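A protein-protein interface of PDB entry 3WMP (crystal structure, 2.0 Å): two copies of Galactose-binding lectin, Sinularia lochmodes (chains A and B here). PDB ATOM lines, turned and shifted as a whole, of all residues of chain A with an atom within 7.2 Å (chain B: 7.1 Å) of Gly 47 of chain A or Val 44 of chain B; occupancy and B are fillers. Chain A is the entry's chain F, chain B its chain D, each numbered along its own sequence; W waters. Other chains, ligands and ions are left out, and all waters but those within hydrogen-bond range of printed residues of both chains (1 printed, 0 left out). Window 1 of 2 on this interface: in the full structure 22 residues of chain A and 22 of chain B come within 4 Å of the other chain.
OG of Ser 45 of chain B is in hydrogen-bond range of OG of Ser 45 of chain A (3.1 Å). The side-chain hydroxyl (OG) of Ser 45 of chain B sits at hydrogen-bond distance from the backbone carbonyl oxygen (O) of Phe 46 of chain A (2.8 Å). The backbone carbonyl oxygen (O) of Val 59 of chain B sits at hydrogen-bond distance from the backbone NH (N) of Leu 49 of chain A, at 2.9 Å. The side-chain hydroxyl (OG) of Ser 61 of chain B is in hydrogen-bond range of the backbone carbonyl oxygen (O) of Gly 47 of chain A (2.8 Å). The side-chain amino group (NZ) of Lys 87 of chain A is in hydrogen-bond range of the backbone carbonyl oxygen (O) of Ser 61 of chain B (2.9 Å).
The backbone NH (N) of Ile 43 of chain B lies within hydrogen-bond range of the backbone carbonyl oxygen (O) of Ile 91 of chain B (3.1 Å). O of Val 44 of chain B is in hydrogen-bond range of OG of Ser 61 of chain B, at 3.3 Å. The backbone carbonyl oxygen (O) of Ser 45 of chain B lies within hydrogen-bond range of the backbone NH (N) of Ile 89 of chain B (2.9 Å). N of Ile 89 of chain A is in hydrogen-bond range of O of Ser 45 of chain A. The backbone NH of Gly 47 of chain A sits at hydrogen-bond distance from the backbone carbonyl oxygen of Lys 87 of chain A, at 2.8 Å. The side-chain sulfur (SD) of Met 48 of chain A sits close to the backbone NH (N) of Tyr 86 of chain A, at 3.7 Å.
Among the printed residues, merely in contact across the chains: Met 10 of chain A with Val 42 of chain B (3.9 Å), Met 10 of chain A with Ile 43 of chain B (3.8 Å), Met 10 of chain A with Ile 91 of chain B (3.9 Å), Thr 12 of chain A with Ile 43 of chain B (3.9 Å), Gly 47 of chain A with Val 44 of chain B (3.6 Å), Gly 47 of chain A with Phe 46 of chain B (3.6 Å), Gly 47 of chain A with Asn 60 of chain B (3.7 Å), Met 48 of chain A with Val 59 of chain B (3.3 Å), Met 48 of chain A with Asn 60 of chain B (3.2 Å), Ile 89 of chain A with Ile 43 of chain B (3.8 Å), Ile 89 of chain A with Val 44 of chain B (3.9 Å) and Ile 89 of chain A with Ser 45 of chain B (3.8 Å).
Printed residues of chain B within 4 Å of Phe 46 of chain A: Ser 45 (2.8 Å). Printed residues of chain B within 4 Å of Gly 47 of chain A: Val 44 (3.6 Å), Phe 46 (3.6 Å), Asn 60 (3.7 Å) and Ser 61 (2.8 Å). Of chain A, only Gly 47 (3.6 Å) and Ile 89 (3.9 Å) come within 4 Å of Val 44 of chain B. Of the printed residues of chain A, Phe 46 of chain B touches Gly 47 (3.6 Å). Of the printed residues of chain A, Val 59 of chain B touches Met 48 (3.3 Å) and Leu 49 (2.9 Å). Leu 73 of chain B touches none of the printed residues of chain A.
Of the 11 printed residues of chain A, 9 touch a printed residue of chain B.
Ser 45 of chain A touches its own counterpart, Ser 45 of chain B. Phe 46 of chain A touches Ser 45 of chain B, but with the chains exchanged Ser 45 of chain A does not touch Phe 46 of chain B (5.4 Å). Ile 89 of chain A touches Ser 45 of chain B, but with the chains exchanged Ser 45 of chain A does not touch Ile 89 of chain B (6.2 Å). Of the 17 pairs that touch across the chains among the printed residues, 1 has its exchanged pair printed and touching as well.
Water W1 lies within hydrogen-bond range of O of Val 44 of chain B (2.7 Å), O of Ser 61 of chain B (2.7 Å) and NZ of Lys 87 of chain A (3.1 Å).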
ATOM      1  N   MET A  10      34.108  -6.782 -34.480  1.00  0.00           N
ATOM      2  CA  MET A  10      33.152  -7.595 -33.756  1.00  0.00           C
ATOM      3  C   MET A  10      31.754  -7.149 -34.114  1.00  0.00           C
ATOM      4  O   MET A  10      31.573  -6.080 -34.695  1.00  0.00           O
ATOM      5  CB  MET A  10      33.392  -7.502 -32.247  1.00  0.00           C
ATOM      6  CG  MET A  10      33.156  -6.134 -31.671  1.00  0.00           C
ATOM      7  SD  MET A  10      33.597  -6.048 -29.920  1.00  0.00           S
ATOM      8  CE  MET A  10      35.283  -5.518 -30.048  1.00  0.00           C
ATOM      9  N   THR A  12      27.119  -8.251 -33.558  1.00  0.00           N
ATOM     10  CA  THR A  12      26.059  -9.087 -33.015  1.00  0.00           C
ATOM     11  C   THR A  12      24.947  -9.266 -34.053  1.00  0.00           C
ATOM     12  O   THR A  12      24.860  -8.499 -35.012  1.00  0.00           O
ATOM     13  CB  THR A  12      25.434  -8.488 -31.717  1.00  0.00           C
ATOM     14  OG1 THR A  12      24.665  -7.324 -32.038  1.00  0.00           O
ATOM     15  CG2 THR A  12      26.519  -8.117 -30.722  1.00  0.00           C
ATOM     16  N   SER A  45      29.529 -16.635 -29.920  1.00  0.00           N
ATOM     17  CA  SER A  45      28.790 -17.061 -28.740  1.00  0.00           C
ATOM     18  C   SER A  45      27.362 -16.497 -28.751  1.00  0.00           C
ATOM     19  O   SER A  45      26.927 -15.928 -29.756  1.00  0.00           O
ATOM     20  CB  SER A  45      29.508 -16.649 -27.458  1.00  0.00           C
ATOM     21  OG  SER A  45      28.951 -17.333 -26.347  1.00  0.00           O
ATOM     22  N   PHE A  46      26.640 -16.660 -27.641  1.00  0.00           N
ATOM     23  CA  PHE A  46      25.270 -16.175 -27.531  1.00  0.00           C
ATOM     24  C   PHE A  46      25.142 -15.027 -26.519  1.00  0.00           C
ATOM     25  O   PHE A  46      25.532 -15.159 -25.364  1.00  0.00           O
ATOM     26  CB  PHE A  46      24.329 -17.318 -27.109  1.00  0.00           C
ATOM     27  CG  PHE A  46      24.182 -18.400 -28.140  1.00  0.00           C
ATOM     28  CD1 PHE A  46      23.133 -18.378 -29.056  1.00  0.00           C
ATOM     29  CD2 PHE A  46      25.109 -19.429 -28.209  1.00  0.00           C
ATOM     30  CE1 PHE A  46      23.016 -19.376 -30.023  1.00  0.00           C
ATOM     31  CE2 PHE A  46      24.998 -20.425 -29.169  1.00  0.00           C
ATOM     32  CZ  PHE A  46      23.952 -20.399 -30.078  1.00  0.00           C
ATOM     33  N   GLY A  47      24.598 -13.898 -26.972  1.00  0.00           N
ATOM     34  CA  GLY A  47      24.380 -12.759 -26.088  1.00  0.00           C
ATOM     35  C   GLY A  47      22.973 -12.744 -25.500  1.00  0.00           C
ATOM     36  O   GLY A  47      22.723 -12.113 -24.468  1.00  0.00           O
ATOM     37  N   MET A  48      22.046 -13.417 -26.177  1.00  0.00           N
ATOM     38  CA  MET A  48      20.675 -13.534 -25.701  1.00  0.00           C
ATOM     39  C   MET A  48      20.176 -14.905 -26.130  1.00  0.00           C
ATOM     40  O   MET A  48      20.586 -15.422 -27.170  1.00  0.00           O
ATOM     41  CB  MET A  48      19.797 -12.392 -26.248  1.00  0.00           C
ATOM     42  CG  MET A  48      18.298 -12.487 -25.937  1.00  0.00           C
ATOM     43  SD  MET A  48      17.362 -13.483 -27.134  1.00  0.00           S
ATOM     44  CE  MET A  48      17.312 -12.340 -28.524  1.00  0.00           C
ATOM     45  N   LEU A  49      19.309 -15.499 -25.311  1.00  0.00           N
ATOM     46  CA  LEU A  49      18.781 -16.829 -25.590  1.00  0.00           C
ATOM     47  C   LEU A  49      17.415 -17.058 -24.944  1.00  0.00           C
ATOM     48  O   LEU A  49      17.169 -16.654 -23.801  1.00  0.00           O
ATOM     49  CB  LEU A  49      19.796 -17.880 -25.105  1.00  0.00           C
ATOM     50  CG  LEU A  49      19.683 -19.308 -25.656  1.00  0.00           C
ATOM     51  CD1 LEU A  49      19.637 -19.292 -27.183  1.00  0.00           C
ATOM     52  CD2 LEU A  49      20.862 -20.143 -25.161  1.00  0.00           C
ATOM     53  N   TYR A  86      17.153 -15.681 -30.143  1.00  0.00           N
ATOM     54  CA  TYR A  86      18.562 -15.736 -29.772  1.00  0.00           C
ATOM     55  C   TYR A  86      19.344 -14.598 -30.413  1.00  0.00           C
ATOM     56  O   TYR A  86      18.931 -14.065 -31.436  1.00  0.00           O
ATOM     57  CB  TYR A  86      19.228 -17.061 -30.166  1.00  0.00           C
ATOM     58  CG  TYR A  86      19.300 -17.301 -31.657  1.00  0.00           C
ATOM     59  CD1 TYR A  86      20.414 -16.912 -32.395  1.00  0.00           C
ATOM     60  CD2 TYR A  86      18.250 -17.918 -32.330  1.00  0.00           C
ATOM     61  CE1 TYR A  86      20.486 -17.141 -33.762  1.00  0.00           C
ATOM     62  CE2 TYR A  86      18.310 -18.150 -33.704  1.00  0.00           C
ATOM     63  CZ  TYR A  86      19.431 -17.761 -34.413  1.00  0.00           C
ATOM     64  OH  TYR A  86      19.515 -17.976 -35.772  1.00  0.00           O
ATOM     65  N   LYS A  87      20.448 -14.195 -29.793  1.00  0.00           N
ATOM     66  CA  LYS A  87      21.322 -13.214 -30.412  1.00  0.00           C
ATOM     67  C   LYS A  87      22.739 -13.779 -30.414  1.00  0.00           C
ATOM     68  O   LYS A  87      23.234 -14.243 -29.384  1.00  0.00           O
ATOM     69  CB  LYS A  87      21.318 -11.874 -29.684  1.00  0.00           C
ATOM     70  CG  LYS A  87      22.206 -10.820 -30.335  1.00  0.00           C
ATOM     71  CD  LYS A  87      22.148  -9.525 -29.550  1.00  0.00           C
ATOM     72  CE  LYS A  87      22.858  -9.688 -28.218  1.00  0.00           C
ATOM     73  NZ  LYS A  87      22.603  -8.547 -27.296  1.00  0.00           N
ATOM     74  N   LEU A  88      23.371 -13.767 -31.582  1.00  0.00           N
ATOM     75  CA  LEU A  88      24.743 -14.234 -31.688  1.00  0.00           C
ATOM     76  C   LEU A  88      25.689 -13.050 -31.513  1.00  0.00           C
ATOM     77  O   LEU A  88      25.333 -11.904 -31.804  1.00  0.00           O
ATOM     78  CB  LEU A  88      25.021 -14.860 -33.080  1.00  0.00           C
ATOM     79  CG  LEU A  88      24.142 -16.050 -33.506  1.00  0.00           C
ATOM     80  CD1 LEU A  88      24.426 -16.429 -34.962  1.00  0.00           C
ATOM     81  CD2 LEU A  88      24.359 -17.240 -32.575  1.00  0.00           C
ATOM     82  N   ILE A  89      26.877 -13.338 -30.988  1.00  0.00           N
ATOM     83  CA  ILE A  89      27.913 -12.330 -30.876  1.00  0.00           C
ATOM     84  C   ILE A  89      29.170 -12.947 -31.487  1.00  0.00           C
ATOM     85  O   ILE A  89      29.348 -14.157 -31.449  1.00  0.00           O
ATOM     86  CB  ILE A  89      28.194 -11.891 -29.431  1.00  0.00           C
ATOM     87  CG1 ILE A  89      28.613 -13.088 -28.582  1.00  0.00           C
ATOM     88  CG2 ILE A  89      26.954 -11.223 -28.856  1.00  0.00           C
ATOM     89  CD1 ILE A  89      29.785 -12.810 -27.672  1.00  0.00           C
ATOM     90  N   VAL B  42      31.705  -3.070 -28.261  1.00  0.00           N
ATOM     91  CA  VAL B  42      31.698  -3.953 -27.114  1.00  0.00           C
ATOM     92  C   VAL B  42      30.656  -5.049 -27.306  1.00  0.00           C
ATOM     93  O   VAL B  42      29.548  -4.767 -27.754  1.00  0.00           O
ATOM     94  CB  VAL B  42      31.335  -3.205 -25.788  1.00  0.00           C
ATOM     95  CG1 VAL B  42      31.595  -4.112 -24.581  1.00  0.00           C
ATOM     96  CG2 VAL B  42      32.125  -1.910 -25.686  1.00  0.00           C
ATOM     97  N   ILE B  43      31.038  -6.301 -27.025  1.00  0.00           N
ATOM     98  CA  ILE B  43      30.086  -7.411 -27.059  1.00  0.00           C
ATOM     99  C   ILE B  43      30.081  -8.064 -25.675  1.00  0.00           C
ATOM    100  O   ILE B  43      31.072  -7.997 -24.948  1.00  0.00           O
ATOM    101  CB  ILE B  43      30.381  -8.463 -28.134  1.00  0.00           C
ATOM    102  CG1 ILE B  43      31.775  -9.056 -27.936  1.00  0.00           C
ATOM    103  CG2 ILE B  43      30.249  -7.834 -29.510  1.00  0.00           C
ATOM    104  CD1 ILE B  43      32.145 -10.102 -28.984  1.00  0.00           C
ATOM    105  N   VAL B  44      28.976  -8.719 -25.344  1.00  0.00           N
ATOM    106  CA  VAL B  44      28.783  -9.321 -24.033  1.00  0.00           C
ATOM    107  C   VAL B  44      28.161 -10.707 -24.132  1.00  0.00           C
ATOM    108  O   VAL B  44      27.286 -10.936 -24.963  1.00  0.00           O
ATOM    109  CB  VAL B  44      27.788  -8.411 -23.196  1.00  0.00           C
ATOM    110  CG1 VAL B  44      27.517  -9.031 -21.836  1.00  0.00           C
ATOM    111  CG2 VAL B  44      28.350  -6.987 -23.068  1.00  0.00           C
ATOM    112  N   SER B  45      28.644 -11.644 -23.327  1.00  0.00           N
ATOM    113  CA  SER B  45      28.038 -12.974 -23.287  1.00  0.00           C
ATOM    114  C   SER B  45      28.000 -13.489 -21.847  1.00  0.00           C
ATOM    115  O   SER B  45      28.171 -12.720 -20.899  1.00  0.00           O
ATOM    116  CB  SER B  45      28.768 -13.984 -24.178  1.00  0.00           C
ATOM    117  OG  SER B  45      28.077 -15.230 -24.180  1.00  0.00           O
ATOM    118  N   PHE B  46      27.783 -14.793 -21.695  1.00  0.00           N
ATOM    119  CA  PHE B  46      27.706 -15.414 -20.386  1.00  0.00           C
ATOM    120  C   PHE B  46      28.817 -16.423 -20.149  1.00  0.00           C
ATOM    121  O   PHE B  46      29.013 -17.341 -20.942  1.00  0.00           O
ATOM    122  CB  PHE B  46      26.349 -16.115 -20.219  1.00  0.00           C
ATOM    123  CG  PHE B  46      25.184 -15.176 -20.199  1.00  0.00           C
ATOM    124  CD1 PHE B  46      24.657 -14.725 -18.997  1.00  0.00           C
ATOM    125  CD2 PHE B  46      24.631 -14.721 -21.386  1.00  0.00           C
ATOM    126  CE1 PHE B  46      23.590 -13.840 -18.985  1.00  0.00           C
ATOM    127  CE2 PHE B  46      23.569 -13.841 -21.381  1.00  0.00           C
ATOM    128  CZ  PHE B  46      23.047 -13.394 -20.180  1.00  0.00           C
ATOM    129  N   VAL B  59      17.463 -15.412 -21.162  1.00  0.00           N
ATOM    130  CA  VAL B  59      18.519 -14.518 -20.692  1.00  0.00           C
ATOM    131  C   VAL B  59      18.925 -13.541 -21.793  1.00  0.00           C
ATOM    132  O   VAL B  59      18.873 -13.861 -22.986  1.00  0.00           O
ATOM    133  CB  VAL B  59      19.781 -15.285 -20.179  1.00  0.00           C
ATOM    134  CG1 VAL B  59      19.421 -16.147 -18.969  1.00  0.00           C
ATOM    135  CG2 VAL B  59      20.377 -16.136 -21.289  1.00  0.00           C
ATOM    136  N   ASN B  60      19.331 -12.344 -21.380  1.00  0.00           N
ATOM    137  CA  ASN B  60      19.727 -11.289 -22.304  1.00  0.00           C
ATOM    138  C   ASN B  60      20.857 -10.445 -21.738  1.00  0.00           C
ATOM    139  O   ASN B  60      20.919 -10.183 -20.536  1.00  0.00           O
ATOM    140  CB  ASN B  60      18.520 -10.372 -22.593  1.00  0.00           C
ATOM    141  CG  ASN B  60      18.806  -9.356 -23.683  1.00  0.00           C
ATOM    142  OD1 ASN B  60      19.506  -9.628 -24.647  1.00  0.00           O
ATOM    143  ND2 ASN B  60      18.226  -8.188 -23.418  1.00  0.00           N
ATOM    144  N   SER B  61      21.758 -10.021 -22.611  1.00  0.00           N
ATOM    145  CA  SER B  61      22.847  -9.169 -22.183  1.00  0.00           C
ATOM    146  C   SER B  61      23.219  -8.181 -23.288  1.00  0.00           C
ATOM    147  O   SER B  61      22.968  -8.434 -24.467  1.00  0.00           O
ATOM    148  CB  SER B  61      24.078 -10.017 -21.817  1.00  0.00           C
ATOM    149  OG  SER B  61      24.621 -10.647 -22.961  1.00  0.00           O
ATOM    150  N   SER B  62      23.775  -7.036 -22.910  1.00  0.00           N
ATOM    151  CA  SER B  62      24.242  -6.075 -23.907  1.00  0.00           C
ATOM    152  C   SER B  62      25.160  -5.029 -23.303  1.00  0.00           C
ATOM    153  O   SER B  62      25.282  -4.929 -22.084  1.00  0.00           O
ATOM    154  CB  SER B  62      23.070  -5.346 -24.583  1.00  0.00           C
ATOM    155  OG  SER B  62      22.202  -4.785 -23.619  1.00  0.00           O
ATOM    156  N   ALA B  63      25.829  -4.279 -24.179  1.00  0.00           N
ATOM    157  CA  ALA B  63      26.676  -3.162 -23.761  1.00  0.00           C
ATOM    158  C   ALA B  63      25.949  -1.884 -24.192  1.00  0.00           C
ATOM    159  O   ALA B  63      25.842  -1.590 -25.382  1.00  0.00           O
ATOM    160  CB  ALA B  63      28.031  -3.233 -24.405  1.00  0.00           C
ATOM    161  N   ASP B  64      25.453  -1.131 -23.216  1.00  0.00           N
ATOM    162  CA  ASP B  64      24.698   0.080 -23.522  1.00  0.00           C
ATOM    163  C   ASP B  64      25.523   1.334 -23.265  1.00  0.00           C
ATOM    164  O   ASP B  64      26.554   1.263 -22.605  1.00  0.00           O
ATOM    165  CB  ASP B  64      23.421   0.113 -22.648  1.00  0.00           C
ATOM    166  CG  ASP B  64      22.523  -1.097 -22.868  1.00  0.00           C
ATOM    167  OD1 ASP B  64      22.503  -1.633 -23.999  1.00  0.00           O
ATOM    168  OD2 ASP B  64      21.820  -1.499 -21.911  1.00  0.00           O
ATOM    169  N   PHE B  71      31.040   2.051 -20.432  1.00  0.00           N
ATOM    170  CA  PHE B  71      29.716   1.628 -20.890  1.00  0.00           C
ATOM    171  C   PHE B  71      28.904   0.992 -19.770  1.00  0.00           C
ATOM    172  O   PHE B  71      29.418   0.776 -18.675  1.00  0.00           O
ATOM    173  CB  PHE B  71      29.863   0.618 -22.050  1.00  0.00           C
ATOM    174  CG  PHE B  71      30.272  -0.762 -21.616  1.00  0.00           C
ATOM    175  CD1 PHE B  71      29.323  -1.771 -21.479  1.00  0.00           C
ATOM    176  CD2 PHE B  71      31.598  -1.047 -21.340  1.00  0.00           C
ATOM    177  CE1 PHE B  71      29.696  -3.046 -21.072  1.00  0.00           C
ATOM    178  CE2 PHE B  71      31.980  -2.317 -20.933  1.00  0.00           C
ATOM    179  CZ  PHE B  71      31.028  -3.320 -20.803  1.00  0.00           C
ATOM    180  N   THR B  72      27.632   0.714 -20.043  1.00  0.00           N
ATOM    181  CA  THR B  72      26.768   0.066 -19.066  1.00  0.00           C
ATOM    182  C   THR B  72      26.573  -1.413 -19.420  1.00  0.00           C
ATOM    183  O   THR B  72      25.963  -1.758 -20.439  1.00  0.00           O
ATOM    184  CB  THR B  72      25.368   0.749 -18.981  1.00  0.00           C
ATOM    185  OG1 THR B  72      25.536   2.114 -18.585  1.00  0.00           O
ATOM    186  CG2 THR B  72      24.481   0.042 -17.963  1.00  0.00           C
ATOM    187  N   LEU B  73      27.142  -2.271 -18.579  1.00  0.00           N
ATOM    188  CA  LEU B  73      27.009  -3.720 -18.724  1.00  0.00           C
ATOM    189  C   LEU B  73      25.578  -4.091 -18.295  1.00  0.00           C
ATOM    190  O   LEU B  73      25.221  -4.010 -17.114  1.00  0.00           O
ATOM    191  CB  LEU B  73      28.051  -4.432 -17.849  1.00  0.00           C
ATOM    192  CG  LEU B  73      28.102  -5.968 -17.911  1.00  0.00           C
ATOM    193  CD1 LEU B  73      28.417  -6.418 -19.333  1.00  0.00           C
ATOM    194  CD2 LEU B  73      29.126  -6.516 -16.916  1.00  0.00           C
ATOM    195  N   HIS B  74      24.766  -4.482 -19.272  1.00  0.00           N
ATOM    196  CA  HIS B  74      23.373  -4.813 -19.030  1.00  0.00           C
ATOM    197  C   HIS B  74      23.019  -6.289 -19.108  1.00  0.00           C
ATOM    198  O   HIS B  74      23.515  -7.027 -19.972  1.00  0.00           O
ATOM    199  CB  HIS B  74      22.477  -4.069 -20.044  1.00  0.00           C
ATOM    200  CG  HIS B  74      21.039  -4.496 -20.010  1.00  0.00           C
ATOM    201  ND1 HIS B  74      20.201  -4.208 -18.952  1.00  0.00           N
ATOM    202  CD2 HIS B  74      20.297  -5.202 -20.896  1.00  0.00           C
ATOM    203  CE1 HIS B  74      19.006  -4.721 -19.188  1.00  0.00           C
ATOM    204  NE2 HIS B  74      19.038  -5.330 -20.361  1.00  0.00           N
ATOM    205  N   TYR B  75      22.170  -6.702 -18.177  1.00  0.00           N
ATOM    206  CA  TYR B  75      21.615  -8.038 -18.167  1.00  0.00           C
ATOM    207  C   TYR B  75      20.118  -7.969 -17.843  1.00  0.00           C
ATOM    208  O   TYR B  75      19.668  -7.056 -17.150  1.00  0.00           O
ATOM    209  CB  TYR B  75      22.261  -8.918 -17.076  1.00  0.00           C
ATOM    210  CG  TYR B  75      21.401 -10.085 -16.631  1.00  0.00           C
ATOM    211  CD1 TYR B  75      21.446 -11.306 -17.302  1.00  0.00           C
ATOM    212  CD2 TYR B  75      20.529  -9.963 -15.545  1.00  0.00           C
ATOM    213  CE1 TYR B  75      20.649 -12.373 -16.902  1.00  0.00           C
ATOM    214  CE2 TYR B  75      19.730 -11.021 -15.142  1.00  0.00           C
ATOM    215  CZ  TYR B  75      19.796 -12.225 -15.824  1.00  0.00           C
ATOM    216  OH  TYR B  75      19.010 -13.283 -15.428  1.00  0.00           O
ATOM    217  N   LEU B  88      28.610 -12.650 -16.383  1.00  0.00           N
ATOM    218  CA  LEU B  88      28.732 -11.983 -17.660  1.00  0.00           C
ATOM    219  C   LEU B  88      30.203 -11.806 -18.039  1.00  0.00           C
ATOM    220  O   LEU B  88      31.074 -11.660 -17.180  1.00  0.00           O
ATOM    221  CB  LEU B  88      28.103 -10.570 -17.602  1.00  0.00           C
ATOM    222  CG  LEU B  88      26.612 -10.479 -17.233  1.00  0.00           C
ATOM    223  CD1 LEU B  88      26.182  -9.019 -17.104  1.00  0.00           C
ATOM    224  CD2 LEU B  88      25.763 -11.206 -18.277  1.00  0.00           C
ATOM    225  N   ILE B  89      30.473 -11.886 -19.337  1.00  0.00           N
ATOM    226  CA  ILE B  89      31.804 -11.584 -19.823  1.00  0.00           C
ATOM    227  C   ILE B  89      31.647 -10.514 -20.908  1.00  0.00           C
ATOM    228  O   ILE B  89      30.615 -10.432 -21.560  1.00  0.00           O
ATOM    229  CB  ILE B  89      32.534 -12.796 -20.422  1.00  0.00           C
ATOM    230  CG1 ILE B  89      31.733 -13.376 -21.587  1.00  0.00           C
ATOM    231  CG2 ILE B  89      32.706 -13.851 -19.348  1.00  0.00           C
ATOM    232  CD1 ILE B  89      32.579 -13.890 -22.709  1.00  0.00           C
ATOM    233  N   TRP B  90      32.660  -9.676 -21.077  1.00  0.00           N
ATOM    234  CA  TRP B  90      32.599  -8.666 -22.108  1.00  0.00           C
ATOM    235  C   TRP B  90      33.991  -8.312 -22.608  1.00  0.00           C
ATOM    236  O   TRP B  90      34.977  -8.460 -21.890  1.00  0.00           O
ATOM    237  CB  TRP B  90      31.923  -7.379 -21.581  1.00  0.00           C
ATOM    238  CG  TRP B  90      32.635  -6.758 -20.415  1.00  0.00           C
ATOM    239  CD1 TRP B  90      32.384  -6.978 -19.091  1.00  0.00           C
ATOM    240  CD2 TRP B  90      33.728  -5.833 -20.469  1.00  0.00           C
ATOM    241  NE1 TRP B  90      33.253  -6.245 -18.315  1.00  0.00           N
ATOM    242  CE2 TRP B  90      34.088  -5.534 -19.135  1.00  0.00           C
ATOM    243  CE3 TRP B  90      34.441  -5.228 -21.513  1.00  0.00           C
ATOM    244  CZ2 TRP B  90      35.127  -4.657 -18.818  1.00  0.00           C
ATOM    245  CZ3 TRP B  90      35.473  -4.354 -21.195  1.00  0.00           C
ATOM    246  CH2 TRP B  90      35.806  -4.078 -19.856  1.00  0.00           C
ATOM    247  N   ILE B  91      34.050  -7.890 -23.867  1.00  0.00           N
ATOM    248  CA  ILE B  91      35.280  -7.406 -24.465  1.00  0.00           C
ATOM    249  C   ILE B  91      34.961  -6.172 -25.323  1.00  0.00           C
ATOM    250  O   ILE B  91      33.936  -6.122 -26.008  1.00  0.00           O
ATOM    251  CB  ILE B  91      36.018  -8.497 -25.308  1.00  0.00           C
ATOM    252  CG1 ILE B  91      37.327  -7.932 -25.879  1.00  0.00           C
ATOM    253  CG2 ILE B  91      35.106  -9.043 -26.395  1.00  0.00           C
ATOM    254  CD1 ILE B  91      38.251  -9.019 -26.425  1.00  0.00           C
HETATM  255  O   HOH W   1      25.145  -9.498 -25.707  1.00  0.00           O
